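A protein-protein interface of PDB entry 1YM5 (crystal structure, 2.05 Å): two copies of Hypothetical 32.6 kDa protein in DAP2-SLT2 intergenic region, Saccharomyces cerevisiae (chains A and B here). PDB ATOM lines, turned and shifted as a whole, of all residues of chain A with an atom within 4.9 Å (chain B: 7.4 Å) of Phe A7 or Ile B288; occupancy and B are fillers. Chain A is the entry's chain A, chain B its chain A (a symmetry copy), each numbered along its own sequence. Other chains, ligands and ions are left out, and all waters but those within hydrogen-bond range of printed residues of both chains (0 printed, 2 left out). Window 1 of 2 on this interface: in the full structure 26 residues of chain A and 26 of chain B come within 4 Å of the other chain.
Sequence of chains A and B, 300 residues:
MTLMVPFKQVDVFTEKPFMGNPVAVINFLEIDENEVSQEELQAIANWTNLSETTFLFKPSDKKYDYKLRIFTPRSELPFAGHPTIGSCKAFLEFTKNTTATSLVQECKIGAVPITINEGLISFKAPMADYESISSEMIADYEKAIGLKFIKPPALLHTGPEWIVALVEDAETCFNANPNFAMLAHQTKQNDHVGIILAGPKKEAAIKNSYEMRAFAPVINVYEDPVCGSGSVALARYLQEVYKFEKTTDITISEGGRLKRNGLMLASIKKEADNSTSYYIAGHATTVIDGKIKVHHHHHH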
ATOM      1  N   VAL A   5      22.074  13.107  -6.151  1.00  0.00           N
ATOM      2  CA  VAL A   5      20.692  13.515  -6.409  1.00  0.00           C
ATOM      3  C   VAL A   5      19.734  12.735  -5.468  1.00  0.00           C
ATOM      4  O   VAL A   5      20.079  11.668  -4.949  1.00  0.00           O
ATOM      5  CB  VAL A   5      20.305  13.280  -7.880  1.00  0.00           C
ATOM      6  CG1 VAL A   5      21.268  13.970  -8.845  1.00  0.00           C
ATOM      7  CG2 VAL A   5      20.264  11.815  -8.209  1.00  0.00           C
ATOM      8  N   PRO A   6      18.541  13.274  -5.235  1.00  0.00           N
ATOM      9  CA  PRO A   6      17.679  12.543  -4.312  1.00  0.00           C
ATOM     10  C   PRO A   6      17.321  11.138  -4.814  1.00  0.00           C
ATOM     11  O   PRO A   6      17.152  10.892  -6.024  1.00  0.00           O
ATOM     12  CB  PRO A   6      16.449  13.427  -4.212  1.00  0.00           C
ATOM     13  CG  PRO A   6      16.953  14.816  -4.569  1.00  0.00           C
ATOM     14  CD  PRO A   6      17.961  14.564  -5.642  1.00  0.00           C
ATOM     15  N   PHE A   7      17.152  10.255  -3.843  1.00  0.00           N
ATOM     16  CA  PHE A   7      16.879   8.871  -4.073  1.00  0.00           C
ATOM     17  C   PHE A   7      15.873   8.345  -3.035  1.00  0.00           C
ATOM     18  O   PHE A   7      15.930   8.655  -1.849  1.00  0.00           O
ATOM     19  CB  PHE A   7      18.210   8.082  -3.987  1.00  0.00           C
ATOM     20  CG  PHE A   7      18.020   6.577  -3.982  1.00  0.00           C
ATOM     21  CD1 PHE A   7      18.035   5.873  -5.137  1.00  0.00           C
ATOM     22  CD2 PHE A   7      17.813   5.893  -2.800  1.00  0.00           C
ATOM     23  CE1 PHE A   7      17.818   4.438  -5.129  1.00  0.00           C
ATOM     24  CE2 PHE A   7      17.581   4.513  -2.816  1.00  0.00           C
ATOM     25  CZ  PHE A   7      17.587   3.803  -4.002  1.00  0.00           C
ATOM     26  N   LYS A   8      14.923   7.568  -3.510  1.00  0.00           N
ATOM     27  CA  LYS A   8      13.983   6.857  -2.638  1.00  0.00           C
ATOM     28  C   LYS A   8      13.840   5.433  -3.096  1.00  0.00           C
ATOM     29  O   LYS A   8      13.751   5.195  -4.292  1.00  0.00           O
ATOM     30  CB  LYS A   8      12.595   7.504  -2.678  1.00  0.00           C
ATOM     31  CG  LYS A   8      12.597   8.929  -2.079  1.00  0.00           C
ATOM     32  CD  LYS A   8      11.282   9.625  -2.191  1.00  0.00           C
ATOM     33  CE  LYS A   8      11.330  11.052  -1.571  1.00  0.00           C
ATOM     34  NZ  LYS A   8      11.013  10.976  -0.106  1.00  0.00           N
ATOM     35  N   GLN A   9      13.826   4.501  -2.134  1.00  0.00           N
ATOM     36  CA  GLN A   9      13.463   3.121  -2.428  1.00  0.00           C
ATOM     37  C   GLN A   9      12.079   2.878  -1.823  1.00  0.00           C
ATOM     38  O   GLN A   9      11.912   2.897  -0.609  1.00  0.00           O
ATOM     39  CB  GLN A   9      14.528   2.160  -1.901  1.00  0.00           C
ATOM     40  CG  GLN A   9      14.470   0.823  -2.553  1.00  0.00           C
ATOM     41  CD  GLN A   9      15.763   0.083  -2.514  1.00  0.00           C
ATOM     42  OE1 GLN A   9      16.766   0.564  -3.064  1.00  0.00           O
ATOM     43  NE2 GLN A   9      15.738  -1.148  -1.948  1.00  0.00           N
ATOM     44  N   ALA A  24      13.638   1.208  -6.847  1.00  0.00           N
ATOM     45  CA  ALA A  24      14.596   2.302  -6.570  1.00  0.00           C
ATOM     46  C   ALA A  24      14.228   3.402  -7.500  1.00  0.00           C
ATOM     47  O   ALA A  24      14.074   3.137  -8.721  1.00  0.00           O
ATOM     48  CB  ALA A  24      16.020   1.876  -6.872  1.00  0.00           C
ATOM     49  N   VAL A  25      14.113   4.636  -6.989  1.00  0.00           N
ATOM     50  CA  VAL A  25      13.688   5.722  -7.844  1.00  0.00           C
ATOM     51  C   VAL A  25      14.698   6.875  -7.734  1.00  0.00           C
ATOM     52  O   VAL A  25      14.883   7.419  -6.648  1.00  0.00           O
ATOM     53  CB  VAL A  25      12.274   6.290  -7.484  1.00  0.00           C
ATOM     54  CG1 VAL A  25      11.876   7.374  -8.473  1.00  0.00           C
ATOM     55  CG2 VAL A  25      11.187   5.227  -7.418  1.00  0.00           C
ATOM     56  N   ILE A  26      15.350   7.197  -8.848  1.00  0.00           N
ATOM     57  CA  ILE A  26      16.346   8.272  -8.910  1.00  0.00           C
ATOM     58  C   ILE A  26      15.746   9.608  -9.436  1.00  0.00           C
ATOM     59  O   ILE A  26      15.054   9.657 -10.473  1.00  0.00           O
ATOM     60  CB  ILE A  26      17.574   7.893  -9.760  1.00  0.00           C
ATOM     61  CG1 ILE A  26      18.379   6.764  -9.099  1.00  0.00           C
ATOM     62  CG2 ILE A  26      18.544   9.107  -9.892  1.00  0.00           C
ATOM     63  CD1 ILE A  26      17.776   5.468  -9.213  1.00  0.00           C
ATOM     64  N   TRP A  47      23.231  -2.500 -10.959  1.00  0.00           N
ATOM     65  CA  TRP A  47      23.826  -2.451  -9.617  1.00  0.00           C
ATOM     66  C   TRP A  47      22.835  -2.533  -8.451  1.00  0.00           C
ATOM     67  O   TRP A  47      23.118  -3.141  -7.405  1.00  0.00           O
ATOM     68  CB  TRP A  47      24.655  -1.160  -9.518  1.00  0.00           C
ATOM     69  CG  TRP A  47      25.385  -1.022  -8.220  1.00  0.00           C
ATOM     70  CD1 TRP A  47      26.591  -1.571  -7.905  1.00  0.00           C
ATOM     71  CD2 TRP A  47      25.000  -0.230  -7.080  1.00  0.00           C
ATOM     72  NE1 TRP A  47      26.973  -1.191  -6.650  1.00  0.00           N
ATOM     73  CE2 TRP A  47      26.011  -0.378  -6.113  1.00  0.00           C
ATOM     74  CE3 TRP A  47      23.882   0.566  -6.774  1.00  0.00           C
ATOM     75  CZ2 TRP A  47      25.951   0.254  -4.869  1.00  0.00           C
ATOM     76  CZ3 TRP A  47      23.835   1.194  -5.540  1.00  0.00           C
ATOM     77  CH2 TRP A  47      24.859   1.043  -4.616  1.00  0.00           C
ATOM     78  N   PHE A  94       9.327  13.809  -3.647  1.00  0.00           N
ATOM     79  CA  PHE A  94      10.426  14.610  -4.134  1.00  0.00           C
ATOM     80  C   PHE A  94      10.005  16.075  -4.339  1.00  0.00           C
ATOM     81  O   PHE A  94      10.773  16.947  -4.024  1.00  0.00           O
ATOM     82  CB  PHE A  94      10.991  14.082  -5.434  1.00  0.00           C
ATOM     83  CG  PHE A  94      11.795  12.811  -5.302  1.00  0.00           C
ATOM     84  CD1 PHE A  94      12.780  12.665  -4.338  1.00  0.00           C
ATOM     85  CD2 PHE A  94      11.654  11.817  -6.250  1.00  0.00           C
ATOM     86  CE1 PHE A  94      13.545  11.516  -4.289  1.00  0.00           C
ATOM     87  CE2 PHE A  94      12.445  10.676  -6.212  1.00  0.00           C
ATOM     88  CZ  PHE A  94      13.392  10.527  -5.231  1.00  0.00           C
ATOM     89  N   ILE A 288      13.546   3.605   2.116  1.00  0.00           N
ATOM     90  CA  ILE A 288      14.863   4.258   2.143  1.00  0.00           C
ATOM     91  C   ILE A 288      14.700   5.610   1.503  1.00  0.00           C
ATOM     92  O   ILE A 288      14.203   5.717   0.385  1.00  0.00           O
ATOM     93  CB  ILE A 288      15.887   3.464   1.362  1.00  0.00           C
ATOM     94  CG1 ILE A 288      16.028   2.080   1.989  1.00  0.00           C
ATOM     95  CG2 ILE A 288      17.234   4.187   1.348  1.00  0.00           C
ATOM     96  CD1 ILE A 288      16.866   1.117   1.221  1.00  0.00           C
ATOM     97  N   ASP A 289      15.096   6.638   2.253  1.00  0.00           N
ATOM     98  CA  ASP A 289      15.078   7.984   1.791  1.00  0.00           C
ATOM     99  C   ASP A 289      16.471   8.656   1.880  1.00  0.00           C
ATOM    100  O   ASP A 289      17.145   8.581   2.891  1.00  0.00           O
ATOM    101  CB  ASP A 289      14.003   8.789   2.552  1.00  0.00           C
ATOM    102  CG  ASP A 289      13.886  10.203   2.015  1.00  0.00           C
ATOM    103  OD1 ASP A 289      13.471  10.345   0.853  1.00  0.00           O
ATOM    104  OD2 ASP A 289      14.257  11.154   2.741  1.00  0.00           O
ATOM    105  N   GLY A 290      16.923   9.294   0.814  1.00  0.00           N
ATOM    106  CA  GLY A 290      18.267   9.878   0.891  1.00  0.00           C
ATOM    107  C   GLY A 290      18.719  10.415  -0.444  1.00  0.00           C
ATOM    108  O   GLY A 290      17.921  11.021  -1.162  1.00  0.00           O
ATOM    109  N   LYS A 291      19.988  10.163  -0.764  1.00  0.00           N
ATOM    110  CA  LYS A 291      20.572  10.630  -1.991  1.00  0.00           C
ATOM    111  C   LYS A 291      21.453   9.544  -2.561  1.00  0.00           C
ATOM    112  O   LYS A 291      21.896   8.692  -1.838  1.00  0.00           O
ATOM    113  CB  LYS A 291      21.451  11.856  -1.688  1.00  0.00           C
ATOM    114  CG  LYS A 291      20.583  13.047  -1.305  1.00  0.00           C
ATOM    115  CD  LYS A 291      21.423  14.199  -1.024  1.00  0.00           C
ATOM    116  CE  LYS A 291      20.591  15.396  -0.665  1.00  0.00           C
ATOM    117  NZ  LYS A 291      19.625  15.685  -1.754  1.00  0.00           N
ATOM    118  N   ILE A 292      21.752   9.638  -3.848  1.00  0.00           N
ATOM    119  CA  ILE A 292      22.576   8.659  -4.532  1.00  0.00           C
ATOM    120  C   ILE A 292      23.619   9.382  -5.342  1.00  0.00           C
ATOM    121  O   ILE A 292      23.318  10.353  -5.983  1.00  0.00           O
ATOM    122  CB  ILE A 292      21.683   7.762  -5.462  1.00  0.00           C
ATOM    123  CG1 ILE A 292      22.474   6.591  -6.054  1.00  0.00           C
ATOM    124  CG2 ILE A 292      20.991   8.573  -6.607  1.00  0.00           C
ATOM    125  CD1 ILE A 292      21.592   5.505  -6.580  1.00  0.00           C
ATOM    126  N   PHE B   7      21.238   4.767   7.068  1.00  0.00           N
ATOM    127  CA  PHE B   7      21.428   3.725   6.109  1.00  0.00           C
ATOM    128  C   PHE B   7      22.431   4.169   5.030  1.00  0.00           C
ATOM    129  O   PHE B   7      22.423   5.297   4.550  1.00  0.00           O
ATOM    130  CB  PHE B   7      20.059   3.384   5.468  1.00  0.00           C
ATOM    131  CG  PHE B   7      20.166   2.458   4.271  1.00  0.00           C
ATOM    132  CD1 PHE B   7      20.082   1.116   4.424  1.00  0.00           C
ATOM    133  CD2 PHE B   7      20.367   2.962   3.001  1.00  0.00           C
ATOM    134  CE1 PHE B   7      20.220   0.234   3.280  1.00  0.00           C
ATOM    135  CE2 PHE B   7      20.523   2.094   1.915  1.00  0.00           C
ATOM    136  CZ  PHE B   7      20.445   0.723   2.081  1.00  0.00           C
ATOM    137  N   LYS B   8      23.325   3.266   4.681  1.00  0.00           N
ATOM    138  CA  LYS B   8      24.247   3.469   3.561  1.00  0.00           C
ATOM    139  C   LYS B   8      24.300   2.229   2.713  1.00  0.00           C
ATOM    140  O   LYS B   8      24.343   1.135   3.255  1.00  0.00           O
ATOM    141  CB  LYS B   8      25.667   3.757   4.059  1.00  0.00           C
ATOM    142  CG  LYS B   8      25.759   5.101   4.817  1.00  0.00           C
ATOM    143  CD  LYS B   8      27.107   5.365   5.401  1.00  0.00           C
ATOM    144  CE  LYS B   8      27.153   6.729   6.149  1.00  0.00           C
ATOM    145  NZ  LYS B   8      27.505   7.823   5.183  1.00  0.00           N
ATOM    146  N   GLN B   9      24.288   2.419   1.387  1.00  0.00           N
ATOM    147  CA  GLN B   9      24.567   1.324   0.467  1.00  0.00           C
ATOM    148  C   GLN B   9      25.951   1.578  -0.132  1.00  0.00           C
ATOM    149  O   GLN B   9      26.152   2.539  -0.866  1.00  0.00           O
ATOM    150  CB  GLN B   9      23.465   1.211  -0.586  1.00  0.00           C
ATOM    151  CG  GLN B   9      23.432  -0.124  -1.244  1.00  0.00           C
ATOM    152  CD  GLN B   9      22.103  -0.474  -1.817  1.00  0.00           C
ATOM    153  OE1 GLN B   9      21.113  -0.560  -1.074  1.00  0.00           O
ATOM    154  NE2 GLN B   9      22.076  -0.780  -3.137  1.00  0.00           N
ATOM    155  N   VAL B  10      26.909   0.752   0.292  1.00  0.00           N
ATOM    156  CA  VAL B  10      28.316   0.916   0.055  1.00  0.00           C
ATOM    157  C   VAL B  10      28.758  -0.044  -1.025  1.00  0.00           C
ATOM    158  O   VAL B  10      28.453  -1.251  -0.960  1.00  0.00           O
ATOM    159  CB  VAL B  10      29.097   0.621   1.302  1.00  0.00           C
ATOM    160  CG1 VAL B  10      30.585   0.890   1.108  1.00  0.00           C
ATOM    161  CG2 VAL B  10      28.558   1.528   2.441  1.00  0.00           C
ATOM    162  N   ASP B  11      29.470   0.500  -2.018  1.00  0.00           N
ATOM    163  CA  ASP B  11      29.988  -0.282  -3.121  1.00  0.00           C
ATOM    164  C   ASP B  11      31.382  -0.770  -2.737  1.00  0.00           C
ATOM    165  O   ASP B  11      32.287   0.045  -2.454  1.00  0.00           O
ATOM    166  CB  ASP B  11      30.029   0.607  -4.381  1.00  0.00           C
ATOM    167  CG  ASP B  11      29.798  -0.152  -5.666  1.00  0.00           C
ATOM    168  OD1 ASP B  11      30.005   0.474  -6.748  1.00  0.00           O
ATOM    169  OD2 ASP B  11      29.458  -1.367  -5.611  1.00  0.00           O
ATOM    170  N   PHE B  18      28.903   2.250  -8.532  1.00  0.00           N
ATOM    171  CA  PHE B  18      28.307   1.291  -9.452  1.00  0.00           C
ATOM    172  C   PHE B  18      29.321   0.308 -10.105  1.00  0.00           C
ATOM    173  O   PHE B  18      28.927  -0.569 -10.871  1.00  0.00           O
ATOM    174  CB  PHE B  18      27.398   1.943 -10.511  1.00  0.00           C
ATOM    175  CG  PHE B  18      26.496   3.010  -9.972  1.00  0.00           C
ATOM    176  CD1 PHE B  18      25.431   2.677  -9.156  1.00  0.00           C
ATOM    177  CD2 PHE B  18      26.751   4.343 -10.230  1.00  0.00           C
ATOM    178  CE1 PHE B  18      24.645   3.647  -8.606  1.00  0.00           C
ATOM    179  CE2 PHE B  18      25.918   5.330  -9.733  1.00  0.00           C
ATOM    180  CZ  PHE B  18      24.890   4.986  -8.874  1.00  0.00           C
ATOM    181  N   VAL B  23      26.752  -3.571  -0.621  1.00  0.00           N
ATOM    182  CA  VAL B  23      26.253  -4.086   0.628  1.00  0.00           C
ATOM    183  C   VAL B  23      25.376  -2.963   1.229  1.00  0.00           C
ATOM    184  O   VAL B  23      25.761  -1.785   1.193  1.00  0.00           O
ATOM    185  CB  VAL B  23      27.394  -4.557   1.586  1.00  0.00           C
ATOM    186  CG1 VAL B  23      28.320  -3.430   1.999  1.00  0.00           C
ATOM    187  CG2 VAL B  23      26.810  -5.216   2.862  1.00  0.00           C
ATOM    188  N   VAL B  25      23.879  -1.317   4.477  1.00  0.00           N
ATOM    189  CA  VAL B  25      24.340  -1.352   5.847  1.00  0.00           C
ATOM    190  C   VAL B  25      23.398  -0.505   6.717  1.00  0.00           C
ATOM    191  O   VAL B  25      23.272   0.694   6.487  1.00  0.00           O
ATOM    192  CB  VAL B  25      25.792  -0.798   6.037  1.00  0.00           C
ATOM    193  CG1 VAL B  25      26.222  -0.939   7.488  1.00  0.00           C
ATOM    194  CG2 VAL B  25      26.820  -1.455   5.127  1.00  0.00           C
ATOM    195  N   GLU B  93      31.949   6.355   8.529  1.00  0.00           N
ATOM    196  CA  GLU B  93      31.095   7.450   8.137  1.00  0.00           C
ATOM    197  C   GLU B  93      29.965   7.719   9.128  1.00  0.00           C
ATOM    198  O   GLU B  93      29.737   8.868   9.521  1.00  0.00           O
ATOM    199  CB  GLU B  93      30.557   7.160   6.750  1.00  0.00           C
ATOM    200  CG  GLU B  93      31.619   7.235   5.676  1.00  0.00           C
ATOM    201  CD  GLU B  93      31.114   7.177   4.239  1.00  0.00           C
ATOM    202  OE1 GLU B  93      29.909   6.976   3.965  1.00  0.00           O
ATOM    203  OE2 GLU B  93      31.954   7.392   3.338  1.00  0.00           O
ATOM    204  N   THR B 285      33.113   2.666  -1.437  1.00  0.00           N
ATOM    205  CA  THR B 285      32.564   4.031  -1.588  1.00  0.00           C
ATOM    206  C   THR B 285      31.069   4.001  -1.317  1.00  0.00           C
ATOM    207  O   THR B 285      30.330   3.171  -1.864  1.00  0.00           O
ATOM    208  CB  THR B 285      32.914   4.658  -2.981  1.00  0.00           C
ATOM    209  OG1 THR B 285      32.557   6.056  -2.969  1.00  0.00           O
ATOM    210  CG2 THR B 285      32.135   4.063  -4.053  1.00  0.00           C
ATOM    211  N   THR B 286      30.601   4.887  -0.440  1.00  0.00           N
ATOM    212  CA  THR B 286      29.177   4.958  -0.171  1.00  0.00           C
ATOM    213  C   THR B 286      28.497   5.524  -1.408  1.00  0.00           C
ATOM    214  O   THR B 286      28.933   6.530  -1.900  1.00  0.00           O
ATOM    215  CB  THR B 286      28.904   5.813   1.089  1.00  0.00           C
ATOM    216  OG1 THR B 286      29.526   5.185   2.219  1.00  0.00           O
ATOM    217  CG2 THR B 286      27.435   5.952   1.330  1.00  0.00           C
ATOM    218  N   VAL B 287      27.437   4.881  -1.891  1.00  0.00           N
ATOM    219  CA  VAL B 287      26.772   5.305  -3.100  1.00  0.00           C
ATOM    220  C   VAL B 287      25.380   5.896  -2.795  1.00  0.00           C
ATOM    221  O   VAL B 287      24.985   6.892  -3.398  1.00  0.00           O
ATOM    222  CB  VAL B 287      26.606   4.098  -4.066  1.00  0.00           C
ATOM    223  CG1 VAL B 287      25.808   4.426  -5.338  1.00  0.00           C
ATOM    224  CG2 VAL B 287      28.002   3.576  -4.467  1.00  0.00           C
ATOM    225  N   ILE B 288      24.633   5.213  -1.932  1.00  0.00           N
ATOM    226  CA  ILE B 288      23.354   5.705  -1.398  1.00  0.00           C
ATOM    227  C   ILE B 288      23.574   6.017   0.058  1.00  0.00           C
ATOM    228  O   ILE B 288      24.046   5.172   0.814  1.00  0.00           O
ATOM    229  CB  ILE B 288      22.268   4.660  -1.519  1.00  0.00           C
ATOM    230  CG1 ILE B 288      22.068   4.317  -2.993  1.00  0.00           C
ATOM    231  CG2 ILE B 288      20.963   5.164  -0.903  1.00  0.00           C
ATOM    232  CD1 ILE B 288      21.158   3.168  -3.260  1.00  0.00           C
ATOM    233  N   ASP B 289      23.256   7.259   0.421  1.00  0.00           N
ATOM    234  CA  ASP B 289      23.335   7.716   1.766  1.00  0.00           C
ATOM    235  C   ASP B 289      21.984   8.273   2.280  1.00  0.00           C
ATOM    236  O   ASP B 289      21.334   9.063   1.619  1.00  0.00           O
ATOM    237  CB  ASP B 289      24.472   8.749   1.907  1.00  0.00           C
ATOM    238  CG  ASP B 289      24.652   9.183   3.349  1.00  0.00           C
ATOM    239  OD1 ASP B 289      25.043   8.329   4.162  1.00  0.00           O
ATOM    240  OD2 ASP B 289      24.353  10.358   3.665  1.00  0.00           O
ATOM    241  N   GLY B 290      21.538   7.845   3.449  1.00  0.00           N
ATOM    242  CA  GLY B 290      20.232   8.336   3.899  1.00  0.00           C
ATOM    243  C   GLY B 290      19.774   7.635   5.154  1.00  0.00           C
ATOM    244  O   GLY B 290      20.584   7.394   6.050  1.00  0.00           O
ATOM    245  N   LYS B 291      18.484   7.298   5.185  1.00  0.00           N
ATOM    246  CA  LYS B 291      17.895   6.646   6.321  1.00  0.00           C
ATOM    247  C   LYS B 291      16.940   5.581   5.837  1.00  0.00           C
ATOM    248  O   LYS B 291      16.471   5.655   4.732  1.00  0.00           O
ATOM    249  CB  LYS B 291      17.092   7.682   7.127  1.00  0.00           C
ATOM    250  CG  LYS B 291      18.034   8.665   7.810  1.00  0.00           C
ATOM    251  CD  LYS B 291      17.266   9.637   8.570  1.00  0.00           C
ATOM    252  CE  LYS B 291      18.172  10.605   9.273  1.00  0.00           C
ATOM    253  NZ  LYS B 291      19.123   9.870  10.142  1.00  0.00           N
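OD2 of Asp B11 sits at hydrogen-bond distance from NE1 of Trp A47.
N of Lys B291 is in hydrogen-bond range of O of Asp A289 (2.9 Å).
The backbone NH (N) of Lys A291 sits at hydrogen-bond distance from the backbone carbonyl oxygen (O) of Asp B289 (2.9 Å).
N of Ile A292 lies within hydrogen-bond range of O of Val A5 (2.9 Å).
The backbone NH of Phe B7 is in hydrogen-bond range of the backbone carbonyl oxygen of Gly B290 (2.9 Å).
The side-chain amino group of Lys B8 lies within salt-bridge range of the side-chain carboxylate of Asp B289.
N of Val B287 lies within hydrogen-bond range of O of Gln B9 (2.9 Å).
The backbone NH of Gln B9 is in hydrogen-bond range of the backbone carbonyl oxygen of Ile B288, 2.8 Å away.
The backbone carbonyl oxygen (O) of Thr B285 lies within hydrogen-bond range of the backbone NH (N) of Asp B11 (2.8 Å).
Among the printed residues, pairs that only touch across the chains: Phe A7 with Ile B288 (3.7 Å), Trp A47 with Gln B9 (3.6 Å), Trp A47 with Phe B18 (3.5 Å), Trp A47 with Val B287 (3.6 Å), Ile A288 with Phe B7 (3.7 Å), Ile A288 with Lys B291 (3.4 Å), Asp A289 with Gly B290 (3.3 Å), Gly A290 with Asp B289 (3.3 Å), Gly A290 with Gly B290 (3.9 Å), Lys A291 with Val B287 (3.9 Å), Lys A291 with Ile B288 (3.4 Å), Ile A292 with Val B287 (3.2 Å) and Ile A292 with Ile B288 (3.8 Å).
Of the printed residues of chain B, Phe A7 touches Ile B288.
Of the printed residues of chain A, Ile B288 touches Phe A7, Lys A291 and Ile A292.
Of the printed residues of chain A, Asp B289 touches Gly A290 (3.3 Å) and Lys A291 (2.9 Å).
Of the printed residues of chain B, Asp A289 touches Gly B290 (3.3 Å) and Lys B291 (2.9 Å).
Printed residues of chain B within 4 Å of Ile A288: Phe B7 (3.7 Å) and Lys B291 (3.4 Å).
Printed residues of chain B within 4 Å of Gly A290: Asp B289 and Gly B290.
Printed residues of chain A within 4 Å of Gln B9: Trp A47.
Val B25 touches none of the printed residues of chain A.
The nearest residue of chain A that does not touch Ile B288 is Trp A47 (4.03 Å).
The nearest printed residue of chain A that does not touch Asp B11 is Ile A292 (9.7 Å).
Hydrophobic or aromatic side chains of chain A within 4 Å of the printed part of chain B: Phe A7, Trp A47, Ile A288 and Ile A292.
Of the 16 printed residues of chain B, 9 touch a printed residue of chain A.
Among the printed residues, 16 pairs touch across the chains.
Among the printed residues, no Asp or Glu carboxylate lies within 4 Å of a Lys or Arg side-chain nitrogen of the other chain.
Phe A7 touches Ile B288, and with the chains exchanged Ile A288 touches Phe B7.
Ile A288 touches Lys B291, and with the chains exchanged Lys A291 touches Ile B288.
Asp A289 touches Lys B291, and with the chains exchanged Lys A291 touches Asp B289.
Gly B290 touches its own counterpart, Gly A290.
Positions printed for both chains: 7, 8, 9, 25, 288, 289, 290 and 291.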
